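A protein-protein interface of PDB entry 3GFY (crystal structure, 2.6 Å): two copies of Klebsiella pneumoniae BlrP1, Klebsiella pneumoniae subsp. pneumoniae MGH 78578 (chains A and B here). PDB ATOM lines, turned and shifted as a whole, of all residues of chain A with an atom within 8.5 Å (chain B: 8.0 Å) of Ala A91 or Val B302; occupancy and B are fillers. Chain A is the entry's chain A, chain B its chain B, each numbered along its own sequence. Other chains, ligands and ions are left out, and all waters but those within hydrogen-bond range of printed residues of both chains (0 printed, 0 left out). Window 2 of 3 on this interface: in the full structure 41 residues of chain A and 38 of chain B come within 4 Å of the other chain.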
ATOM      1  N   MET A   9      15.244  17.686 -33.848  1.00  0.00           N
ATOM      2  CA  MET A   9      16.193  17.535 -32.701  1.00  0.00           C
ATOM      3  C   MET A   9      17.381  18.481 -32.848  1.00  0.00           C
ATOM      4  O   MET A   9      18.320  18.198 -33.595  1.00  0.00           O
ATOM      5  CB  MET A   9      16.692  16.089 -32.599  1.00  0.00           C
ATOM      6  CG  MET A   9      15.635  15.081 -32.157  1.00  0.00           C
ATOM      7  SD  MET A   9      15.284  15.154 -30.384  1.00  0.00           S
ATOM      8  CE  MET A   9      16.866  14.659 -29.698  1.00  0.00           C
ATOM      9  N   LEU A  10      17.338  19.596 -32.123  1.00  0.00           N
ATOM     10  CA  LEU A  10      18.378  20.619 -32.218  1.00  0.00           C
ATOM     11  C   LEU A  10      19.723  20.164 -31.650  1.00  0.00           C
ATOM     12  O   LEU A  10      19.784  19.490 -30.624  1.00  0.00           O
ATOM     13  CB  LEU A  10      17.924  21.909 -31.534  1.00  0.00           C
ATOM     14  CG  LEU A  10      18.807  23.131 -31.786  1.00  0.00           C
ATOM     15  CD1 LEU A  10      18.587  23.687 -33.192  1.00  0.00           C
ATOM     16  CD2 LEU A  10      18.534  24.182 -30.748  1.00  0.00           C
ATOM     17  N   THR A  11      20.794  20.558 -32.333  1.00  0.00           N
ATOM     18  CA  THR A  11      22.154  20.132 -32.020  1.00  0.00           C
ATOM     19  C   THR A  11      23.108  21.320 -32.212  1.00  0.00           C
ATOM     20  O   THR A  11      22.815  22.243 -32.972  1.00  0.00           O
ATOM     21  CB  THR A  11      22.559  18.933 -32.931  1.00  0.00           C
ATOM     22  OG1 THR A  11      21.631  17.858 -32.742  1.00  0.00           O
ATOM     23  CG2 THR A  11      23.963  18.425 -32.638  1.00  0.00           C
ATOM     24  N   THR A  12      24.227  21.303 -31.500  1.00  0.00           N
ATOM     25  CA  THR A  12      25.276  22.300 -31.658  1.00  0.00           C
ATOM     26  C   THR A  12      26.584  21.615 -32.068  1.00  0.00           C
ATOM     27  O   THR A  12      27.018  20.661 -31.423  1.00  0.00           O
ATOM     28  CB  THR A  12      25.489  23.093 -30.347  1.00  0.00           C
ATOM     29  OG1 THR A  12      24.328  23.884 -30.069  1.00  0.00           O
ATOM     30  CG2 THR A  12      26.706  24.006 -30.444  1.00  0.00           C
ATOM     31  N   GLU A  60      24.401  25.457 -35.535  1.00  0.00           N
ATOM     32  CA  GLU A  60      23.203  25.022 -34.829  1.00  0.00           C
ATOM     33  C   GLU A  60      22.155  24.561 -35.830  1.00  0.00           C
ATOM     34  O   GLU A  60      21.930  25.219 -36.842  1.00  0.00           O
ATOM     35  CB  GLU A  60      22.631  26.157 -33.979  1.00  0.00           C
ATOM     36  CG  GLU A  60      23.578  26.690 -32.926  1.00  0.00           C
ATOM     37  CD  GLU A  60      22.961  27.789 -32.092  1.00  0.00           C
ATOM     38  OE1 GLU A  60      22.607  28.846 -32.659  1.00  0.00           O
ATOM     39  OE2 GLU A  60      22.838  27.596 -30.863  1.00  0.00           O
ATOM     40  N   ASP A  88      26.777  18.108 -29.474  1.00  0.00           N
ATOM     41  CA  ASP A  88      25.869  17.775 -28.392  1.00  0.00           C
ATOM     42  C   ASP A  88      24.452  18.223 -28.736  1.00  0.00           C
ATOM     43  O   ASP A  88      24.270  19.160 -29.514  1.00  0.00           O
ATOM     44  CB  ASP A  88      26.335  18.474 -27.113  1.00  0.00           C
ATOM     45  CG  ASP A  88      26.079  17.654 -25.868  1.00  0.00           C
ATOM     46  OD1 ASP A  88      25.034  16.971 -25.795  1.00  0.00           O
ATOM     47  OD2 ASP A  88      26.929  17.697 -24.956  1.00  0.00           O
ATOM     48  N   TYR A  89      23.456  17.555 -28.157  1.00  0.00           N
ATOM     49  CA  TYR A  89      22.064  17.969 -28.315  1.00  0.00           C
ATOM     50  C   TYR A  89      21.832  19.298 -27.598  1.00  0.00           C
ATOM     51  O   TYR A  89      22.492  19.595 -26.599  1.00  0.00           O
ATOM     52  CB  TYR A  89      21.108  16.892 -27.795  1.00  0.00           C
ATOM     53  CG  TYR A  89      21.113  15.612 -28.606  1.00  0.00           C
ATOM     54  CD1 TYR A  89      20.507  15.553 -29.860  1.00  0.00           C
ATOM     55  CD2 TYR A  89      21.717  14.458 -28.115  1.00  0.00           C
ATOM     56  CE1 TYR A  89      20.510  14.380 -30.608  1.00  0.00           C
ATOM     57  CE2 TYR A  89      21.725  13.280 -28.852  1.00  0.00           C
ATOM     58  CZ  TYR A  89      21.119  13.247 -30.097  1.00  0.00           C
ATOM     59  OH  TYR A  89      21.122  12.074 -30.824  1.00  0.00           O
ATOM     60  N   SER A  90      20.896  20.093 -28.113  1.00  0.00           N
ATOM     61  CA  SER A  90      20.740  21.479 -27.679  1.00  0.00           C
ATOM     62  C   SER A  90      19.297  21.857 -27.353  1.00  0.00           C
ATOM     63  O   SER A  90      18.358  21.471 -28.054  1.00  0.00           O
ATOM     64  CB  SER A  90      21.304  22.423 -28.742  1.00  0.00           C
ATOM     65  OG  SER A  90      21.212  23.769 -28.327  1.00  0.00           O
ATOM     66  N   ALA A  91      19.138  22.631 -26.285  1.00  0.00           N
ATOM     67  CA  ALA A  91      17.828  23.031 -25.789  1.00  0.00           C
ATOM     68  C   ALA A  91      17.244  24.195 -26.576  1.00  0.00           C
ATOM     69  O   ALA A  91      16.037  24.255 -26.807  1.00  0.00           O
ATOM     70  CB  ALA A  91      17.925  23.400 -24.332  1.00  0.00           C
ATOM     71  N   TYR A  92      18.105  25.125 -26.973  1.00  0.00           N
ATOM     72  CA  TYR A  92      17.659  26.321 -27.670  1.00  0.00           C
ATOM     73  C   TYR A  92      18.699  26.824 -28.663  1.00  0.00           C
ATOM     74  O   TYR A  92      19.875  26.476 -28.582  1.00  0.00           O
ATOM     75  CB  TYR A  92      17.275  27.424 -26.673  1.00  0.00           C
ATOM     76  CG  TYR A  92      18.414  27.926 -25.810  1.00  0.00           C
ATOM     77  CD1 TYR A  92      18.822  27.221 -24.677  1.00  0.00           C
ATOM     78  CD2 TYR A  92      19.067  29.118 -26.112  1.00  0.00           C
ATOM     79  CE1 TYR A  92      19.862  27.680 -23.881  1.00  0.00           C
ATOM     80  CE2 TYR A  92      20.106  29.588 -25.318  1.00  0.00           C
ATOM     81  CZ  TYR A  92      20.499  28.862 -24.208  1.00  0.00           C
ATOM     82  OH  TYR A  92      21.531  29.321 -23.423  1.00  0.00           O
ATOM     83  N   ARG A  93      18.239  27.630 -29.611  1.00  0.00           N
ATOM     84  CA  ARG A  93      19.096  28.217 -30.624  1.00  0.00           C
ATOM     85  C   ARG A  93      19.704  29.506 -30.075  1.00  0.00           C
ATOM     86  O   ARG A  93      18.982  30.408 -29.647  1.00  0.00           O
ATOM     87  CB  ARG A  93      18.268  28.500 -31.877  1.00  0.00           C
ATOM     88  CG  ARG A  93      19.065  28.601 -33.150  1.00  0.00           C
ATOM     89  CD  ARG A  93      18.151  28.770 -34.360  1.00  0.00           C
ATOM     90  NE  ARG A  93      17.556  27.513 -34.816  1.00  0.00           N
ATOM     91  CZ  ARG A  93      18.157  26.641 -35.625  1.00  0.00           C
ATOM     92  NH1 ARG A  93      19.386  26.872 -36.066  1.00  0.00           N
ATOM     93  NH2 ARG A  93      17.531  25.529 -35.991  1.00  0.00           N
ATOM     94  N   ARG A  94      21.032  29.582 -30.073  1.00  0.00           N
ATOM     95  CA  ARG A  94      21.731  30.753 -29.552  1.00  0.00           C
ATOM     96  C   ARG A  94      21.859  31.868 -30.582  1.00  0.00           C
ATOM     97  O   ARG A  94      21.875  33.041 -30.226  1.00  0.00           O
ATOM     98  CB  ARG A  94      23.115  30.385 -29.007  1.00  0.00           C
ATOM     99  CG  ARG A  94      23.124  29.907 -27.561  1.00  0.00           C
ATOM    100  CD  ARG A  94      22.650  28.469 -27.445  1.00  0.00           C
ATOM    101  NE  ARG A  94      23.026  27.854 -26.175  1.00  0.00           N
ATOM    102  CZ  ARG A  94      22.644  26.639 -25.794  1.00  0.00           C
ATOM    103  NH1 ARG A  94      21.866  25.905 -26.579  1.00  0.00           N
ATOM    104  NH2 ARG A  94      23.034  26.159 -24.622  1.00  0.00           N
ATOM    105  N   ASP A 131      27.113  28.813 -19.858  1.00  0.00           N
ATOM    106  CA  ASP A 131      26.892  28.044 -21.075  1.00  0.00           C
ATOM    107  C   ASP A 131      28.217  27.603 -21.701  1.00  0.00           C
ATOM    108  O   ASP A 131      29.148  28.406 -21.831  1.00  0.00           O
ATOM    109  CB  ASP A 131      26.075  28.856 -22.079  1.00  0.00           C
ATOM    110  CG  ASP A 131      25.691  28.048 -23.294  1.00  0.00           C
ATOM    111  OD1 ASP A 131      24.929  27.072 -23.142  1.00  0.00           O
ATOM    112  OD2 ASP A 131      26.156  28.388 -24.400  1.00  0.00           O
ATOM    113  N   VAL B 260      12.672  13.698 -15.972  1.00  0.00           N
ATOM    114  CA  VAL B 260      13.082  14.963 -16.573  1.00  0.00           C
ATOM    115  C   VAL B 260      11.868  15.870 -16.720  1.00  0.00           C
ATOM    116  O   VAL B 260      11.903  17.036 -16.317  1.00  0.00           O
ATOM    117  CB  VAL B 260      13.762  14.737 -17.946  1.00  0.00           C
ATOM    118  CG1 VAL B 260      14.090  16.063 -18.617  1.00  0.00           C
ATOM    119  CG2 VAL B 260      15.021  13.889 -17.781  1.00  0.00           C
ATOM    120  N   MET B 264      10.901  19.223 -14.748  1.00  0.00           N
ATOM    121  CA  MET B 264      10.531  20.337 -15.608  1.00  0.00           C
ATOM    122  C   MET B 264       9.282  21.035 -15.073  1.00  0.00           C
ATOM    123  O   MET B 264       9.303  22.238 -14.811  1.00  0.00           O
ATOM    124  CB  MET B 264      10.292  19.825 -17.035  1.00  0.00           C
ATOM    125  CG  MET B 264      10.802  20.713 -18.160  1.00  0.00           C
ATOM    126  SD  MET B 264      12.518  21.253 -17.969  1.00  0.00           S
ATOM    127  CE  MET B 264      12.250  22.948 -17.466  1.00  0.00           C
ATOM    128  N   PRO B 274      14.632  26.348 -16.798  1.00  0.00           N
ATOM    129  CA  PRO B 274      15.452  25.149 -17.018  1.00  0.00           C
ATOM    130  C   PRO B 274      16.960  25.374 -16.895  1.00  0.00           C
ATOM    131  O   PRO B 274      17.632  24.623 -16.191  1.00  0.00           O
ATOM    132  CB  PRO B 274      15.112  24.739 -18.461  1.00  0.00           C
ATOM    133  CG  PRO B 274      14.226  25.829 -19.009  1.00  0.00           C
ATOM    134  CD  PRO B 274      13.587  26.468 -17.829  1.00  0.00           C
ATOM    135  N   ASP B 275      17.476  26.401 -17.565  1.00  0.00           N
ATOM    136  CA  ASP B 275      18.917  26.674 -17.586  1.00  0.00           C
ATOM    137  C   ASP B 275      19.459  27.190 -16.251  1.00  0.00           C
ATOM    138  O   ASP B 275      20.674  27.306 -16.065  1.00  0.00           O
ATOM    139  CB  ASP B 275      19.272  27.638 -18.723  1.00  0.00           C
ATOM    140  CG  ASP B 275      18.505  28.943 -18.645  1.00  0.00           C
ATOM    141  OD1 ASP B 275      17.307  28.955 -19.007  1.00  0.00           O
ATOM    142  OD2 ASP B 275      19.105  29.958 -18.228  1.00  0.00           O
ATOM    143  N   VAL B 296      19.228   9.534 -20.374  1.00  0.00           N
ATOM    144  CA  VAL B 296      18.811  10.452 -19.319  1.00  0.00           C
ATOM    145  C   VAL B 296      19.454  11.828 -19.520  1.00  0.00           C
ATOM    146  O   VAL B 296      18.760  12.846 -19.496  1.00  0.00           O
ATOM    147  CB  VAL B 296      19.110   9.876 -17.905  1.00  0.00           C
ATOM    148  CG1 VAL B 296      19.097  10.968 -16.837  1.00  0.00           C
ATOM    149  CG2 VAL B 296      18.111   8.775 -17.559  1.00  0.00           C
ATOM    150  N   LEU B 297      20.771  11.844 -19.741  1.00  0.00           N
ATOM    151  CA  LEU B 297      21.512  13.090 -19.972  1.00  0.00           C
ATOM    152  C   LEU B 297      21.026  13.773 -21.243  1.00  0.00           C
ATOM    153  O   LEU B 297      20.933  14.997 -21.294  1.00  0.00           O
ATOM    154  CB  LEU B 297      23.025  12.826 -20.041  1.00  0.00           C
ATOM    155  CG  LEU B 297      24.066  13.967 -20.082  1.00  0.00           C
ATOM    156  CD1 LEU B 297      24.492  14.331 -21.509  1.00  0.00           C
ATOM    157  CD2 LEU B 297      23.641  15.225 -19.310  1.00  0.00           C
ATOM    158  N   LYS B 298      20.714  12.968 -22.255  1.00  0.00           N
ATOM    159  CA  LYS B 298      20.165  13.455 -23.515  1.00  0.00           C
ATOM    160  C   LYS B 298      18.903  14.277 -23.277  1.00  0.00           C
ATOM    161  O   LYS B 298      18.794  15.403 -23.761  1.00  0.00           O
ATOM    162  CB  LYS B 298      19.876  12.279 -24.452  1.00  0.00           C
ATOM    163  CG  LYS B 298      19.373  12.662 -25.838  1.00  0.00           C
ATOM    164  CD  LYS B 298      19.313  11.432 -26.741  1.00  0.00           C
ATOM    165  CE  LYS B 298      18.467  11.679 -27.981  1.00  0.00           C
ATOM    166  NZ  LYS B 298      17.031  11.887 -27.629  1.00  0.00           N
ATOM    167  N   ALA B 299      17.971  13.720 -22.508  1.00  0.00           N
ATOM    168  CA  ALA B 299      16.710  14.391 -22.199  1.00  0.00           C
ATOM    169  C   ALA B 299      16.906  15.632 -21.324  1.00  0.00           C
ATOM    170  O   ALA B 299      16.203  16.631 -21.491  1.00  0.00           O
ATOM    171  CB  ALA B 299      15.738  13.422 -21.544  1.00  0.00           C
ATOM    172  N   LEU B 300      17.864  15.559 -20.400  1.00  0.00           N
ATOM    173  CA  LEU B 300      18.204  16.680 -19.524  1.00  0.00           C
ATOM    174  C   LEU B 300      18.817  17.847 -20.293  1.00  0.00           C
ATOM    175  O   LEU B 300      18.558  19.012 -19.982  1.00  0.00           O
ATOM    176  CB  LEU B 300      19.164  16.225 -18.425  1.00  0.00           C
ATOM    177  CG  LEU B 300      18.610  15.370 -17.283  1.00  0.00           C
ATOM    178  CD1 LEU B 300      19.747  14.716 -16.519  1.00  0.00           C
ATOM    179  CD2 LEU B 300      17.729  16.189 -16.350  1.00  0.00           C
ATOM    180  N   ARG B 301      19.634  17.523 -21.291  1.00  0.00           N
ATOM    181  CA  ARG B 301      20.241  18.522 -22.168  1.00  0.00           C
ATOM    182  C   ARG B 301      19.205  19.230 -23.034  1.00  0.00           C
ATOM    183  O   ARG B 301      19.232  20.456 -23.160  1.00  0.00           O
ATOM    184  CB  ARG B 301      21.306  17.877 -23.058  1.00  0.00           C
ATOM    185  CG  ARG B 301      22.650  17.705 -22.388  1.00  0.00           C
ATOM    186  CD  ARG B 301      23.500  18.968 -22.494  1.00  0.00           C
ATOM    187  NE  ARG B 301      24.434  19.083 -21.377  1.00  0.00           N
ATOM    188  CZ  ARG B 301      25.602  18.450 -21.293  1.00  0.00           C
ATOM    189  NH1 ARG B 301      26.006  17.640 -22.266  1.00  0.00           N
ATOM    190  NH2 ARG B 301      26.368  18.625 -20.228  1.00  0.00           N
ATOM    191  N   VAL B 302      18.297  18.451 -23.621  1.00  0.00           N
ATOM    192  CA  VAL B 302      17.251  18.985 -24.497  1.00  0.00           C
ATOM    193  C   VAL B 302      16.257  19.828 -23.697  1.00  0.00           C
ATOM    194  O   VAL B 302      15.735  20.826 -24.195  1.00  0.00           O
ATOM    195  CB  VAL B 302      16.530  17.855 -25.296  1.00  0.00           C
ATOM    196  CG1 VAL B 302      15.361  18.402 -26.112  1.00  0.00           C
ATOM    197  CG2 VAL B 302      17.510  17.147 -26.216  1.00  0.00           C
ATOM    198  N   ALA B 303      16.028  19.440 -22.445  1.00  0.00           N
ATOM    199  CA  ALA B 303      15.190  20.223 -21.539  1.00  0.00           C
ATOM    200  C   ALA B 303      15.836  21.565 -21.195  1.00  0.00           C
ATOM    201  O   ALA B 303      15.144  22.562 -21.006  1.00  0.00           O
ATOM    202  CB  ALA B 303      14.893  19.438 -20.282  1.00  0.00           C
ATOM    203  N   GLY B 304      17.163  21.588 -21.119  1.00  0.00           N
ATOM    204  CA  GLY B 304      17.891  22.830 -20.894  1.00  0.00           C
ATOM    205  C   GLY B 304      18.583  22.928 -19.555  1.00  0.00           C
ATOM    206  O   GLY B 304      19.167  23.957 -19.231  1.00  0.00           O
ATOM    207  N   MET B 305      18.518  21.856 -18.776  1.00  0.00           N
ATOM    208  CA  MET B 305      19.164  21.826 -17.470  1.00  0.00           C
ATOM    209  C   MET B 305      20.647  21.514 -17.614  1.00  0.00           C
ATOM    210  O   MET B 305      21.077  20.944 -18.617  1.00  0.00           O
ATOM    211  CB  MET B 305      18.481  20.808 -16.557  1.00  0.00           C
ATOM    212  CG  MET B 305      17.144  21.277 -16.016  1.00  0.00           C
ATOM    213  SD  MET B 305      16.224  19.986 -15.162  1.00  0.00           S
ATOM    214  CE  MET B 305      15.374  19.197 -16.527  1.00  0.00           C
ATOM    215  N   LYS B 306      21.424  21.902 -16.609  1.00  0.00           N
ATOM    216  CA  LYS B 306      22.862  21.651 -16.604  1.00  0.00           C
ATOM    217  C   LYS B 306      23.186  20.369 -15.845  1.00  0.00           C
ATOM    218  O   LYS B 306      22.385  19.902 -15.033  1.00  0.00           O
ATOM    219  CB  LYS B 306      23.613  22.838 -16.001  1.00  0.00           C
ATOM    220  CG  LYS B 306      23.974  23.938 -16.994  1.00  0.00           C
ATOM    221  CD  LYS B 306      22.789  24.823 -17.348  1.00  0.00           C
ATOM    222  CE  LYS B 306      23.205  25.987 -18.241  1.00  0.00           C
ATOM    223  NZ  LYS B 306      23.740  25.525 -19.553  1.00  0.00           N
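No position is printed for both chains.
The backbone carbonyl oxygen of Met A9 sits at hydrogen-bond distance from the side-chain hydroxyl of Thr A11 (3.4 Å).
The backbone carbonyl oxygen (O) of Asp A88 is in hydrogen-bond range of the backbone NH (N) of Thr A12 (2.9 Å).
The backbone NH (N) of Asp B275 sits close to the backbone carbonyl oxygen (O) of Gly B304.
Among the printed residues, merely in contact across the chains: Ala A91 with Val B302 (3.4 Å), Ala A91 with Arg B301 (3.4 Å), Met A9 with Lys B298 (3.5 Å), Ala A91 with Gly B304 (3.5 Å), Tyr A89 with Lys B298 (3.7 Å) and Tyr A89 with Val B302 (3.9 Å).
Hydrophobic or aromatic side chains of chain A that line the printed part of chain B: Met A9, Tyr A89 and Ala A91.
Along chain B the printed residues that touch a printed residue of chain A span positions 298 to 304.
Among the printed residues, Asp or Glu carboxylates within 4 Å of a Lys or Arg side-chain nitrogen of the other chain: Asp A88 with Arg B301.
Of the printed residues of chain B, Met A9 touches Lys B298 (3.5 Å).
Printed residues of chain B within 4 Å of Asp A88: Arg B301.
Ser A90 touches none of the printed residues of chain B.
Ala A91 touches just these residues of chain B: Arg B301, Val B302 and Gly B304.
Leu B300 touches none of the printed residues of chain A.
Val B302 touches just these residues of chain A: Tyr A89 and Ala A91.
No residue of chain A comes within 4 Å of Ala B303.
The nearest residue of chain A that does not touch Val B302 is Met A9 (4.3 Å).
The nearest printed residue of chain A that does not touch Lys B298 is Asp A88 (6.4 Å).
NH1 of Arg B301 lies within salt-bridge range of OD2 of Asp A88 (2.8 Å).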
